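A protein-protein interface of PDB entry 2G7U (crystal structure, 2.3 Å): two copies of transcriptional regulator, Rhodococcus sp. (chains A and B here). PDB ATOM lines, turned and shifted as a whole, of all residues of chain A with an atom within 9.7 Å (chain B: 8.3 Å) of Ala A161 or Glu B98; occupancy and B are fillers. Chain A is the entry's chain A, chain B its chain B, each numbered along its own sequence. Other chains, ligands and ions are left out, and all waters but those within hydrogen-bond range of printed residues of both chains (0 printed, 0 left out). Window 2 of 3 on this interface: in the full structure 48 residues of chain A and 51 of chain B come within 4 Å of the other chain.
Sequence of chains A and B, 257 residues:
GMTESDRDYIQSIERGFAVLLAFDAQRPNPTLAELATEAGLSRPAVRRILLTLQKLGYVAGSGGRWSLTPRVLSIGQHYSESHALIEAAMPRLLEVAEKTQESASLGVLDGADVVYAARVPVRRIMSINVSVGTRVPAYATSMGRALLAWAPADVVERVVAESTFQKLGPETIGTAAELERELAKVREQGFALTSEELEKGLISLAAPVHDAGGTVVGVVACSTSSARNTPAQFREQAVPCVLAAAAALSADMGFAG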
ATOM      1  N   GLY A 111     -26.985   1.550  15.809  1.00  0.00           N
ATOM      2  CA  GLY A 111     -27.534   0.500  16.672  1.00  0.00           C
ATOM      3  C   GLY A 111     -29.047   0.519  16.612  1.00  0.00           C
ATOM      4  O   GLY A 111     -29.623   0.294  15.540  1.00  0.00           O
ATOM      5  N   ALA A 112     -29.690   0.829  17.749  1.00  0.00           N
ATOM      6  CA  ALA A 112     -31.171   0.883  17.849  1.00  0.00           C
ATOM      7  C   ALA A 112     -31.700   2.317  17.813  1.00  0.00           C
ATOM      8  O   ALA A 112     -32.908   2.561  17.907  1.00  0.00           O
ATOM      9  CB  ALA A 112     -31.651   0.184  19.116  1.00  0.00           C
ATOM     10  N   TYR A 139     -37.325   2.290  16.675  1.00  0.00           N
ATOM     11  CA  TYR A 139     -38.599   1.571  16.699  1.00  0.00           C
ATOM     12  C   TYR A 139     -39.809   2.539  16.735  1.00  0.00           C
ATOM     13  O   TYR A 139     -40.892   2.168  16.312  1.00  0.00           O
ATOM     14  CB  TYR A 139     -38.642   0.585  17.879  1.00  0.00           C
ATOM     15  CG  TYR A 139     -38.926   1.230  19.218  1.00  0.00           C
ATOM     16  CD1 TYR A 139     -40.236   1.536  19.599  1.00  0.00           C
ATOM     17  CD2 TYR A 139     -37.886   1.541  20.103  1.00  0.00           C
ATOM     18  CE1 TYR A 139     -40.501   2.138  20.818  1.00  0.00           C
ATOM     19  CE2 TYR A 139     -38.140   2.154  21.330  1.00  0.00           C
ATOM     20  CZ  TYR A 139     -39.448   2.445  21.681  1.00  0.00           C
ATOM     21  OH  TYR A 139     -39.721   3.044  22.888  1.00  0.00           O
ATOM     22  N   LEU A 148     -34.918   1.066   8.415  1.00  0.00           N
ATOM     23  CA  LEU A 148     -34.936  -0.377   8.656  1.00  0.00           C
ATOM     24  C   LEU A 148     -35.679  -1.169   7.623  1.00  0.00           C
ATOM     25  O   LEU A 148     -35.417  -2.371   7.475  1.00  0.00           O
ATOM     26  CB  LEU A 148     -35.513  -0.693  10.027  1.00  0.00           C
ATOM     27  CG  LEU A 148     -34.690  -0.254  11.241  1.00  0.00           C
ATOM     28  CD1 LEU A 148     -35.538  -0.486  12.468  1.00  0.00           C
ATOM     29  CD2 LEU A 148     -33.369  -1.055  11.311  1.00  0.00           C
ATOM     30  N   ALA A 153     -31.907  -8.583   7.406  1.00  0.00           N
ATOM     31  CA  ALA A 153     -32.579  -9.158   8.568  1.00  0.00           C
ATOM     32  C   ALA A 153     -31.805  -8.974   9.880  1.00  0.00           C
ATOM     33  O   ALA A 153     -32.406  -8.665  10.912  1.00  0.00           O
ATOM     34  CB  ALA A 153     -32.890 -10.642   8.325  1.00  0.00           C
ATOM     35  N   ASP A 154     -30.482  -9.141   9.834  1.00  0.00           N
ATOM     36  CA  ASP A 154     -29.638  -9.035  11.031  1.00  0.00           C
ATOM     37  C   ASP A 154     -29.585  -7.613  11.590  1.00  0.00           C
ATOM     38  O   ASP A 154     -29.429  -7.419  12.799  1.00  0.00           O
ATOM     39  CB  ASP A 154     -28.222  -9.583  10.776  1.00  0.00           C
ATOM     40  CG  ASP A 154     -27.498  -8.851   9.648  1.00  0.00           C
ATOM     41  OD1 ASP A 154     -27.760  -9.173   8.459  1.00  0.00           O
ATOM     42  OD2 ASP A 154     -26.659  -7.968   9.955  1.00  0.00           O
ATOM     43  N   VAL A 155     -29.726  -6.621  10.717  1.00  0.00           N
ATOM     44  CA  VAL A 155     -29.798  -5.229  11.164  1.00  0.00           C
ATOM     45  C   VAL A 155     -31.120  -4.950  11.882  1.00  0.00           C
ATOM     46  O   VAL A 155     -31.136  -4.328  12.950  1.00  0.00           O
ATOM     47  CB  VAL A 155     -29.553  -4.237  10.004  1.00  0.00           C
ATOM     48  CG1 VAL A 155     -29.840  -2.797  10.452  1.00  0.00           C
ATOM     49  CG2 VAL A 155     -28.086  -4.365   9.483  1.00  0.00           C
ATOM     50  N   VAL A 156     -32.224  -5.444  11.326  1.00  0.00           N
ATOM     51  CA  VAL A 156     -33.524  -5.317  11.988  1.00  0.00           C
ATOM     52  C   VAL A 156     -33.492  -6.077  13.319  1.00  0.00           C
ATOM     53  O   VAL A 156     -33.941  -5.565  14.351  1.00  0.00           O
ATOM     54  CB  VAL A 156     -34.684  -5.801  11.086  1.00  0.00           C
ATOM     55  CG1 VAL A 156     -36.015  -5.648  11.798  1.00  0.00           C
ATOM     56  CG2 VAL A 156     -34.712  -5.024   9.761  1.00  0.00           C
ATOM     57  N   GLU A 157     -32.911  -7.272  13.290  1.00  0.00           N
ATOM     58  CA  GLU A 157     -32.775  -8.129  14.460  1.00  0.00           C
ATOM     59  C   GLU A 157     -32.017  -7.436  15.610  1.00  0.00           C
ATOM     60  O   GLU A 157     -32.396  -7.573  16.776  1.00  0.00           O
ATOM     61  CB  GLU A 157     -32.075  -9.434  14.051  1.00  0.00           C
ATOM     62  CG  GLU A 157     -32.622 -10.706  14.671  1.00  0.00           C
ATOM     63  CD  GLU A 157     -31.898 -11.998  14.192  1.00  0.00           C
ATOM     64  OE1 GLU A 157     -32.352 -13.097  14.609  1.00  0.00           O
ATOM     65  OE2 GLU A 157     -30.888 -11.939  13.422  1.00  0.00           O
ATOM     66  N   ARG A 158     -30.959  -6.686  15.292  1.00  0.00           N
ATOM     67  CA  ARG A 158     -30.200  -5.982  16.336  1.00  0.00           C
ATOM     68  C   ARG A 158     -31.048  -4.915  17.026  1.00  0.00           C
ATOM     69  O   ARG A 158     -31.169  -4.883  18.260  1.00  0.00           O
ATOM     70  CB  ARG A 158     -28.894  -5.393  15.792  1.00  0.00           C
ATOM     71  CG  ARG A 158     -28.252  -4.349  16.733  1.00  0.00           C
ATOM     72  CD  ARG A 158     -26.773  -4.547  16.902  1.00  0.00           C
ATOM     73  NE  ARG A 158     -25.986  -3.643  16.071  1.00  0.00           N
ATOM     74  CZ  ARG A 158     -25.209  -2.660  16.535  1.00  0.00           C
ATOM     75  NH1 ARG A 158     -25.114  -2.424  17.843  1.00  0.00           N
ATOM     76  NH2 ARG A 158     -24.520  -1.907  15.679  1.00  0.00           N
ATOM     77  N   VAL A 159     -31.641  -4.044  16.222  1.00  0.00           N
ATOM     78  CA  VAL A 159     -32.585  -3.068  16.717  1.00  0.00           C
ATOM     79  C   VAL A 159     -33.580  -3.679  17.688  1.00  0.00           C
ATOM     80  O   VAL A 159     -33.703  -3.193  18.817  1.00  0.00           O
ATOM     81  CB  VAL A 159     -33.336  -2.412  15.572  1.00  0.00           C
ATOM     82  CG1 VAL A 159     -34.459  -1.543  16.108  1.00  0.00           C
ATOM     83  CG2 VAL A 159     -32.358  -1.588  14.744  1.00  0.00           C
ATOM     84  N   VAL A 160     -34.266  -4.746  17.263  1.00  0.00           N
ATOM     85  CA  VAL A 160     -35.255  -5.409  18.093  1.00  0.00           C
ATOM     86  C   VAL A 160     -34.678  -5.805  19.456  1.00  0.00           C
ATOM     87  O   VAL A 160     -35.300  -5.550  20.491  1.00  0.00           O
ATOM     88  CB  VAL A 160     -35.826  -6.651  17.388  1.00  0.00           C
ATOM     89  CG1 VAL A 160     -36.730  -7.443  18.332  1.00  0.00           C
ATOM     90  CG2 VAL A 160     -36.568  -6.263  16.103  1.00  0.00           C
ATOM     91  N   ALA A 161     -33.485  -6.401  19.455  1.00  0.00           N
ATOM     92  CA  ALA A 161     -32.851  -6.892  20.681  1.00  0.00           C
ATOM     93  C   ALA A 161     -32.478  -5.768  21.635  1.00  0.00           C
ATOM     94  O   ALA A 161     -32.460  -5.955  22.848  1.00  0.00           O
ATOM     95  CB  ALA A 161     -31.612  -7.733  20.350  1.00  0.00           C
ATOM     96  N   GLU A 162     -32.184  -4.603  21.068  1.00  0.00           N
ATOM     97  CA  GLU A 162     -31.727  -3.441  21.824  1.00  0.00           C
ATOM     98  C   GLU A 162     -32.815  -2.395  22.098  1.00  0.00           C
ATOM     99  O   GLU A 162     -32.537  -1.356  22.695  1.00  0.00           O
ATOM    100  CB  GLU A 162     -30.550  -2.792  21.087  1.00  0.00           C
ATOM    101  CG  GLU A 162     -29.317  -3.702  20.996  1.00  0.00           C
ATOM    102  CD  GLU A 162     -28.096  -3.021  20.376  1.00  0.00           C
ATOM    103  OE1 GLU A 162     -28.120  -1.795  20.100  1.00  0.00           O
ATOM    104  OE2 GLU A 162     -27.098  -3.728  20.164  1.00  0.00           O
ATOM    105  N   SER A 163     -34.048  -2.657  21.676  1.00  0.00           N
ATOM    106  CA  SER A 163     -35.126  -1.678  21.847  1.00  0.00           C
ATOM    107  C   SER A 163     -35.901  -1.927  23.129  1.00  0.00           C
ATOM    108  O   SER A 163     -36.153  -3.080  23.488  1.00  0.00           O
ATOM    109  CB  SER A 163     -36.068  -1.722  20.657  1.00  0.00           C
ATOM    110  OG  SER A 163     -35.393  -1.349  19.467  1.00  0.00           O
ATOM    111  N   THR A 164     -36.279  -0.861  23.831  1.00  0.00           N
ATOM    112  CA  THR A 164     -37.109  -1.036  25.033  1.00  0.00           C
ATOM    113  C   THR A 164     -38.556  -1.288  24.666  1.00  0.00           C
ATOM    114  O   THR A 164     -39.250  -1.995  25.380  1.00  0.00           O
ATOM    115  CB  THR A 164     -37.042   0.166  26.006  1.00  0.00           C
ATOM    116  OG1 THR A 164     -37.105   1.396  25.264  1.00  0.00           O
ATOM    117  CG2 THR A 164     -35.736   0.126  26.824  1.00  0.00           C
ATOM    118  N   PHE A 165     -38.989  -0.728  23.533  1.00  0.00           N
ATOM    119  CA  PHE A 165     -40.405  -0.720  23.124  1.00  0.00           C
ATOM    120  C   PHE A 165     -41.343  -0.064  24.145  1.00  0.00           C
ATOM    121  O   PHE A 165     -42.512  -0.427  24.242  1.00  0.00           O
ATOM    122  CB  PHE A 165     -40.918  -2.112  22.769  1.00  0.00           C
ATOM    123  CG  PHE A 165     -40.416  -2.639  21.452  1.00  0.00           C
ATOM    124  CD1 PHE A 165     -39.442  -3.635  21.417  1.00  0.00           C
ATOM    125  CD2 PHE A 165     -40.947  -2.173  20.251  1.00  0.00           C
ATOM    126  CE1 PHE A 165     -38.991  -4.148  20.196  1.00  0.00           C
ATOM    127  CE2 PHE A 165     -40.498  -2.669  19.026  1.00  0.00           C
ATOM    128  CZ  PHE A 165     -39.514  -3.653  18.996  1.00  0.00           C
ATOM    129  N   ALA A 176     -42.212  -6.103  18.715  1.00  0.00           N
ATOM    130  CA  ALA A 176     -41.493  -6.535  17.498  1.00  0.00           C
ATOM    131  C   ALA A 176     -42.435  -6.908  16.332  1.00  0.00           C
ATOM    132  O   ALA A 176     -42.152  -6.590  15.178  1.00  0.00           O
ATOM    133  CB  ALA A 176     -40.562  -7.752  17.821  1.00  0.00           C
ATOM    134  N   LEU A 179     -43.707  -3.613  14.931  1.00  0.00           N
ATOM    135  CA  LEU A 179     -42.627  -2.968  14.147  1.00  0.00           C
ATOM    136  C   LEU A 179     -42.482  -3.550  12.738  1.00  0.00           C
ATOM    137  O   LEU A 179     -42.301  -2.820  11.759  1.00  0.00           O
ATOM    138  CB  LEU A 179     -41.284  -3.152  14.842  1.00  0.00           C
ATOM    139  CG  LEU A 179     -40.191  -2.072  14.717  1.00  0.00           C
ATOM    140  CD1 LEU A 179     -38.824  -2.722  14.848  1.00  0.00           C
ATOM    141  CD2 LEU A 179     -40.251  -1.125  13.479  1.00  0.00           C
ATOM    142  N   GLU A 180     -42.526  -4.881  12.689  1.00  0.00           N
ATOM    143  CA  GLU A 180     -42.409  -5.679  11.494  1.00  0.00           C
ATOM    144  C   GLU A 180     -43.554  -5.366  10.518  1.00  0.00           C
ATOM    145  O   GLU A 180     -43.310  -5.168   9.327  1.00  0.00           O
ATOM    146  CB  GLU A 180     -42.437  -7.152  11.903  1.00  0.00           C
ATOM    147  CG  GLU A 180     -41.576  -8.045  11.075  1.00  0.00           C
ATOM    148  CD  GLU A 180     -40.100  -7.942  11.452  1.00  0.00           C
ATOM    149  OE1 GLU A 180     -39.318  -7.384  10.641  1.00  0.00           O
ATOM    150  OE2 GLU A 180     -39.737  -8.420  12.558  1.00  0.00           O
ATOM    151  N   MET B  90     -23.176 -12.745   9.743  1.00  0.00           N
ATOM    152  CA  MET B  90     -23.832 -11.621  10.443  1.00  0.00           C
ATOM    153  C   MET B  90     -24.701 -12.048  11.638  1.00  0.00           C
ATOM    154  O   MET B  90     -24.469 -11.564  12.729  1.00  0.00           O
ATOM    155  CB  MET B  90     -24.671 -10.768   9.463  1.00  0.00           C
ATOM    156  CG  MET B  90     -23.880 -10.102   8.347  1.00  0.00           C
ATOM    157  SD  MET B  90     -22.257  -9.245   9.063  1.00  0.00           S
ATOM    158  CE  MET B  90     -22.925  -7.868  10.214  1.00  0.00           C
ATOM    159  N   PRO B  91     -25.717 -12.930  11.421  1.00  0.00           N
ATOM    160  CA  PRO B  91     -26.567 -13.429  12.525  1.00  0.00           C
ATOM    161  C   PRO B  91     -25.776 -14.133  13.626  1.00  0.00           C
ATOM    162  O   PRO B  91     -26.113 -13.986  14.799  1.00  0.00           O
ATOM    163  CB  PRO B  91     -27.546 -14.408  11.842  1.00  0.00           C
ATOM    164  CG  PRO B  91     -26.991 -14.670  10.438  1.00  0.00           C
ATOM    165  CD  PRO B  91     -26.122 -13.477  10.100  1.00  0.00           C
ATOM    166  N   ARG B  92     -24.718 -14.854  13.268  1.00  0.00           N
ATOM    167  CA  ARG B  92     -23.872 -15.490  14.273  1.00  0.00           C
ATOM    168  C   ARG B  92     -23.072 -14.465  15.074  1.00  0.00           C
ATOM    169  O   ARG B  92     -22.915 -14.616  16.288  1.00  0.00           O
ATOM    170  CB  ARG B  92     -22.879 -16.472  13.639  1.00  0.00           C
ATOM    171  CG  ARG B  92     -23.482 -17.561  12.796  1.00  0.00           C
ATOM    172  CD  ARG B  92     -24.727 -18.113  13.408  1.00  0.00           C
ATOM    173  NE  ARG B  92     -25.383 -19.085  12.531  1.00  0.00           N
ATOM    174  CZ  ARG B  92     -26.379 -19.872  12.926  1.00  0.00           C
ATOM    175  NH1 ARG B  92     -26.834 -19.795  14.167  1.00  0.00           N
ATOM    176  NH2 ARG B  92     -26.910 -20.748  12.096  1.00  0.00           N
ATOM    177  N   LEU B  93     -22.524 -13.452  14.401  1.00  0.00           N
ATOM    178  CA  LEU B  93     -21.817 -12.391  15.112  1.00  0.00           C
ATOM    179  C   LEU B  93     -22.754 -11.589  16.025  1.00  0.00           C
ATOM    180  O   LEU B  93     -22.348 -11.166  17.095  1.00  0.00           O
ATOM    181  CB  LEU B  93     -21.126 -11.432  14.137  1.00  0.00           C
ATOM    182  CG  LEU B  93     -20.065 -11.949  13.166  1.00  0.00           C
ATOM    183  CD1 LEU B  93     -19.589 -10.775  12.319  1.00  0.00           C
ATOM    184  CD2 LEU B  93     -18.901 -12.649  13.848  1.00  0.00           C
ATOM    185  N   LEU B  94     -24.001 -11.379  15.597  1.00  0.00           N
ATOM    186  CA  LEU B  94     -24.991 -10.698  16.438  1.00  0.00           C
ATOM    187  C   LEU B  94     -25.240 -11.476  17.720  1.00  0.00           C
ATOM    188  O   LEU B  94     -25.398 -10.868  18.786  1.00  0.00           O
ATOM    189  CB  LEU B  94     -26.322 -10.449  15.697  1.00  0.00           C
ATOM    190  CG  LEU B  94     -27.434  -9.757  16.485  1.00  0.00           C
ATOM    191  CD1 LEU B  94     -26.991  -8.391  17.008  1.00  0.00           C
ATOM    192  CD2 LEU B  94     -28.755  -9.611  15.684  1.00  0.00           C
ATOM    193  N   GLU B  95     -25.302 -12.802  17.628  1.00  0.00           N
ATOM    194  CA  GLU B  95     -25.514 -13.632  18.820  1.00  0.00           C
ATOM    195  C   GLU B  95     -24.357 -13.434  19.813  1.00  0.00           C
ATOM    196  O   GLU B  95     -24.591 -13.257  21.009  1.00  0.00           O
ATOM    197  CB  GLU B  95     -25.685 -15.121  18.464  1.00  0.00           C
ATOM    198  CG  GLU B  95     -26.995 -15.472  17.774  1.00  0.00           C
ATOM    199  CD  GLU B  95     -26.979 -16.830  17.015  1.00  0.00           C
ATOM    200  OE1 GLU B  95     -26.005 -17.617  17.146  1.00  0.00           O
ATOM    201  OE2 GLU B  95     -27.954 -17.099  16.271  1.00  0.00           O
ATOM    202  N   VAL B  96     -23.122 -13.433  19.317  1.00  0.00           N
ATOM    203  CA  VAL B  96     -21.953 -13.132  20.144  1.00  0.00           C
ATOM    204  C   VAL B  96     -22.013 -11.727  20.764  1.00  0.00           C
ATOM    205  O   VAL B  96     -21.800 -11.558  21.967  1.00  0.00           O
ATOM    206  CB  VAL B  96     -20.602 -13.345  19.356  1.00  0.00           C
ATOM    207  CG1 VAL B  96     -19.359 -12.968  20.206  1.00  0.00           C
ATOM    208  CG2 VAL B  96     -20.463 -14.790  18.872  1.00  0.00           C
ATOM    209  N   ALA B  97     -22.310 -10.716  19.952  1.00  0.00           N
ATOM    210  CA  ALA B  97     -22.331  -9.338  20.463  1.00  0.00           C
ATOM    211  C   ALA B  97     -23.390  -9.185  21.546  1.00  0.00           C
ATOM    212  O   ALA B  97     -23.108  -8.574  22.561  1.00  0.00           O
ATOM    213  CB  ALA B  97     -22.579  -8.318  19.330  1.00  0.00           C
ATOM    214  N   GLU B  98     -24.591  -9.735  21.332  1.00  0.00           N
ATOM    215  CA  GLU B  98     -25.673  -9.640  22.318  1.00  0.00           C
ATOM    216  C   GLU B  98     -25.324 -10.317  23.650  1.00  0.00           C
ATOM    217  O   GLU B  98     -25.607  -9.783  24.723  1.00  0.00           O
ATOM    218  CB  GLU B  98     -26.954 -10.286  21.782  1.00  0.00           C
ATOM    219  CG  GLU B  98     -27.711  -9.537  20.657  1.00  0.00           C
ATOM    220  CD  GLU B  98     -28.809 -10.415  20.017  1.00  0.00           C
ATOM    221  OE1 GLU B  98     -29.472  -9.944  19.056  1.00  0.00           O
ATOM    222  OE2 GLU B  98     -29.019 -11.586  20.465  1.00  0.00           O
ATOM    223  N   LYS B  99     -24.748 -11.512  23.568  1.00  0.00           N
ATOM    224  CA  LYS B  99     -24.474 -12.305  24.742  1.00  0.00           C
ATOM    225  C   LYS B  99     -23.352 -11.677  25.591  1.00  0.00           C
ATOM    226  O   LYS B  99     -23.453 -11.608  26.817  1.00  0.00           O
ATOM    227  CB  LYS B  99     -24.112 -13.736  24.333  1.00  0.00           C
ATOM    228  CG  LYS B  99     -24.901 -14.793  25.097  1.00  0.00           C
ATOM    229  CD  LYS B  99     -23.971 -15.857  25.693  1.00  0.00           C
ATOM    230  CE  LYS B  99     -24.728 -16.828  26.592  1.00  0.00           C
ATOM    231  NZ  LYS B  99     -25.858 -17.529  25.875  1.00  0.00           N
ATOM    232  N   THR B 100     -22.299 -11.200  24.916  1.00  0.00           N
ATOM    233  CA  THR B 100     -21.115 -10.685  25.584  1.00  0.00           C
ATOM    234  C   THR B 100     -21.173  -9.172  25.804  1.00  0.00           C
ATOM    235  O   THR B 100     -20.456  -8.643  26.664  1.00  0.00           O
ATOM    236  CB  THR B 100     -19.850 -10.971  24.787  1.00  0.00           C
ATOM    237  OG1 THR B 100     -19.936 -10.291  23.516  1.00  0.00           O
ATOM    238  CG2 THR B 100     -19.637 -12.499  24.590  1.00  0.00           C
ATOM    239  N   GLN B 101     -22.021  -8.487  25.043  1.00  0.00           N
ATOM    240  CA  GLN B 101     -21.960  -7.025  24.950  1.00  0.00           C
ATOM    241  C   GLN B 101     -20.558  -6.548  24.578  1.00  0.00           C
ATOM    242  O   GLN B 101     -20.114  -5.490  25.033  1.00  0.00           O
ATOM    243  CB  GLN B 101     -22.435  -6.342  26.238  1.00  0.00           C
ATOM    244  CG  GLN B 101     -23.928  -6.518  26.518  1.00  0.00           C
ATOM    245  CD  GLN B 101     -24.818  -6.033  25.376  1.00  0.00           C
ATOM    246  OE1 GLN B 101     -24.709  -4.895  24.933  1.00  0.00           O
ATOM    247  NE2 GLN B 101     -25.723  -6.888  24.925  1.00  0.00           N
ATOM    248  N   GLU B 102     -19.864  -7.340  23.755  1.00  0.00           N
ATOM    249  CA  GLU B 102     -18.588  -6.938  23.155  1.00  0.00           C
ATOM    250  C   GLU B 102     -18.731  -7.076  21.639  1.00  0.00           C
ATOM    251  O   GLU B 102     -19.430  -7.992  21.172  1.00  0.00           O
ATOM    252  CB  GLU B 102     -17.455  -7.835  23.669  1.00  0.00           C
ATOM    253  CG  GLU B 102     -17.193  -7.767  25.196  1.00  0.00           C
ATOM    254  CD  GLU B 102     -16.573  -6.431  25.682  1.00  0.00           C
ATOM    255  OE1 GLU B 102     -16.313  -5.540  24.836  1.00  0.00           O
ATOM    256  OE2 GLU B 102     -16.330  -6.281  26.919  1.00  0.00           O
ATOM    257  N   SER B 103     -18.087  -6.199  20.863  1.00  0.00           N
ATOM    258  CA  SER B 103     -18.208  -6.277  19.407  1.00  0.00           C
ATOM    259  C   SER B 103     -17.652  -7.613  18.923  1.00  0.00           C
ATOM    260  O   SER B 103     -16.590  -8.051  19.405  1.00  0.00           O
ATOM    261  CB  SER B 103     -17.473  -5.125  18.706  1.00  0.00           C
ATOM    262  OG  SER B 103     -17.851  -3.876  19.278  1.00  0.00           O
ATOM    263  N   ALA B 104     -18.380  -8.232  17.985  1.00  0.00           N
ATOM    264  CA  ALA B 104     -18.050  -9.531  17.392  1.00  0.00           C
ATOM    265  C   ALA B 104     -17.639  -9.302  15.940  1.00  0.00           C
ATOM    266  O   ALA B 104     -18.265  -8.492  15.250  1.00  0.00           O
ATOM    267  CB  ALA B 104     -19.279 -10.447  17.439  1.00  0.00           C
ATOM    268  N   VAL B 120     -20.172  -6.660  13.988  1.00  0.00           N
ATOM    269  CA  VAL B 120     -21.342  -6.215  14.734  1.00  0.00           C
ATOM    270  C   VAL B 120     -20.827  -5.457  15.968  1.00  0.00           C
ATOM    271  O   VAL B 120     -20.367  -6.067  16.921  1.00  0.00           O
ATOM    272  CB  VAL B 120     -22.225  -7.396  15.190  1.00  0.00           C
ATOM    273  CG1 VAL B 120     -23.350  -6.885  16.071  1.00  0.00           C
ATOM    274  CG2 VAL B 120     -22.803  -8.132  13.998  1.00  0.00           C
ATOM    275  N   PRO B 121     -20.870  -4.125  15.940  1.00  0.00           N
ATOM    276  CA  PRO B 121     -20.336  -3.353  17.058  1.00  0.00           C
ATOM    277  C   PRO B 121     -21.348  -3.211  18.195  1.00  0.00           C
ATOM    278  O   PRO B 121     -22.562  -3.321  17.980  1.00  0.00           O
ATOM    279  CB  PRO B 121     -20.085  -1.981  16.434  1.00  0.00           C
ATOM    280  CG  PRO B 121     -21.198  -1.859  15.418  1.00  0.00           C
ATOM    281  CD  PRO B 121     -21.399  -3.261  14.869  1.00  0.00           C
ATOM    282  N   VAL B 122     -20.841  -2.987  19.401  1.00  0.00           N
ATOM    283  CA  VAL B 122     -21.691  -2.629  20.519  1.00  0.00           C
ATOM    284  C   VAL B 122     -21.381  -1.173  20.887  1.00  0.00           C
ATOM    285  O   VAL B 122     -20.228  -0.748  20.817  1.00  0.00           O
ATOM    286  CB  VAL B 122     -21.411  -3.525  21.728  1.00  0.00           C
ATOM    287  CG1 VAL B 122     -21.754  -4.997  21.389  1.00  0.00           C
ATOM    288  CG2 VAL B 122     -19.973  -3.365  22.126  1.00  0.00           C
ATOM    289  N   CYS B 222     -14.014 -12.075  19.295  1.00  0.00           N
ATOM    290  CA  CYS B 222     -14.615 -11.157  20.253  1.00  0.00           C
ATOM    291  C   CYS B 222     -13.533 -10.553  21.136  1.00  0.00           C
ATOM    292  O   CYS B 222     -12.652 -11.252  21.598  1.00  0.00           O
ATOM    293  CB  CYS B 222     -15.628 -11.898  21.133  1.00  0.00           C
ATOM    294  SG  CYS B 222     -16.626 -10.858  22.143  1.00  0.00           S
ATOM    295  N   CYS B 241     -19.921 -18.992  23.740  1.00  0.00           N
ATOM    296  CA  CYS B 241     -20.733 -18.461  22.631  1.00  0.00           C
ATOM    297  C   CYS B 241     -19.904 -18.194  21.381  1.00  0.00           C
ATOM    298  O   CYS B 241     -20.444 -18.197  20.276  1.00  0.00           O
ATOM    299  CB  CYS B 241     -21.541 -17.213  23.024  1.00  0.00           C
ATOM    300  SG  CYS B 241     -20.548 -15.707  23.231  1.00  0.00           S
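The guanidinium group (NH1) of Arg A158 sits at hydrogen-bond distance from the backbone carbonyl oxygen (O) of Pro B121 (2.7 Å).
The guanidinium group (NH1) of Arg A158 lies within salt-bridge range of the side-chain carboxylate (OE2) of Glu A162 (3.3 Å).
The backbone carbonyl oxygen (O) of Glu B98 is in hydrogen-bond range of the side-chain amide nitrogen (NE2) of Gln B101, 2.9 Å away.
CB of Met B90 touches CG of Asp A154 (3.4 Å).
O of Asp A154 touches CD2 of Leu B94, 3.7 Å away.
Glu A157 touches Leu B94.
Arg A158 touches Leu B94.
Ala A161 touches Glu B98 (CB to OE1, 3.3 Å).
Of the printed residues of chain B, Asp A154 touches Met B90 and Leu B94.
Val A155 touches none of the printed residues of chain B.
Printed residues of chain B within 4 Å of Glu A157: Leu B94 (3.7 Å).
Printed residues of chain B within 4 Å of Arg A158: Leu B94 (3.7 Å) and Pro B121 (2.7 Å).
Of chain B, only Glu B98 (3.3 Å) comes within 4 Å of Ala A161.
Printed residues of chain A within 4 Å of Met B90: Asp A154.
Of the printed residues of chain A, Leu B94 touches Asp A154, Glu A157 and Arg A158.
Glu B98 touches one residue of chain A.
The nearest residue of chain B that does not touch Ala A161 is Leu B94 (5.7 Å).
The nearest residue of chain A that does not touch Glu B98 is Glu A157 (4.4 Å).
Hydrophobic or aromatic side chains of chain A within 4 Å of the printed part of chain B: Ala A161.
Of the 20 printed residues of chain B, 4 touch a printed residue of chain A.
Among the printed residues, 6 pairs touch across the chains.
No position is printed for both chains.
Of the 6 pairs that touch across the chains among the printed residues, none has its exchanged pair printed and touching as well.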
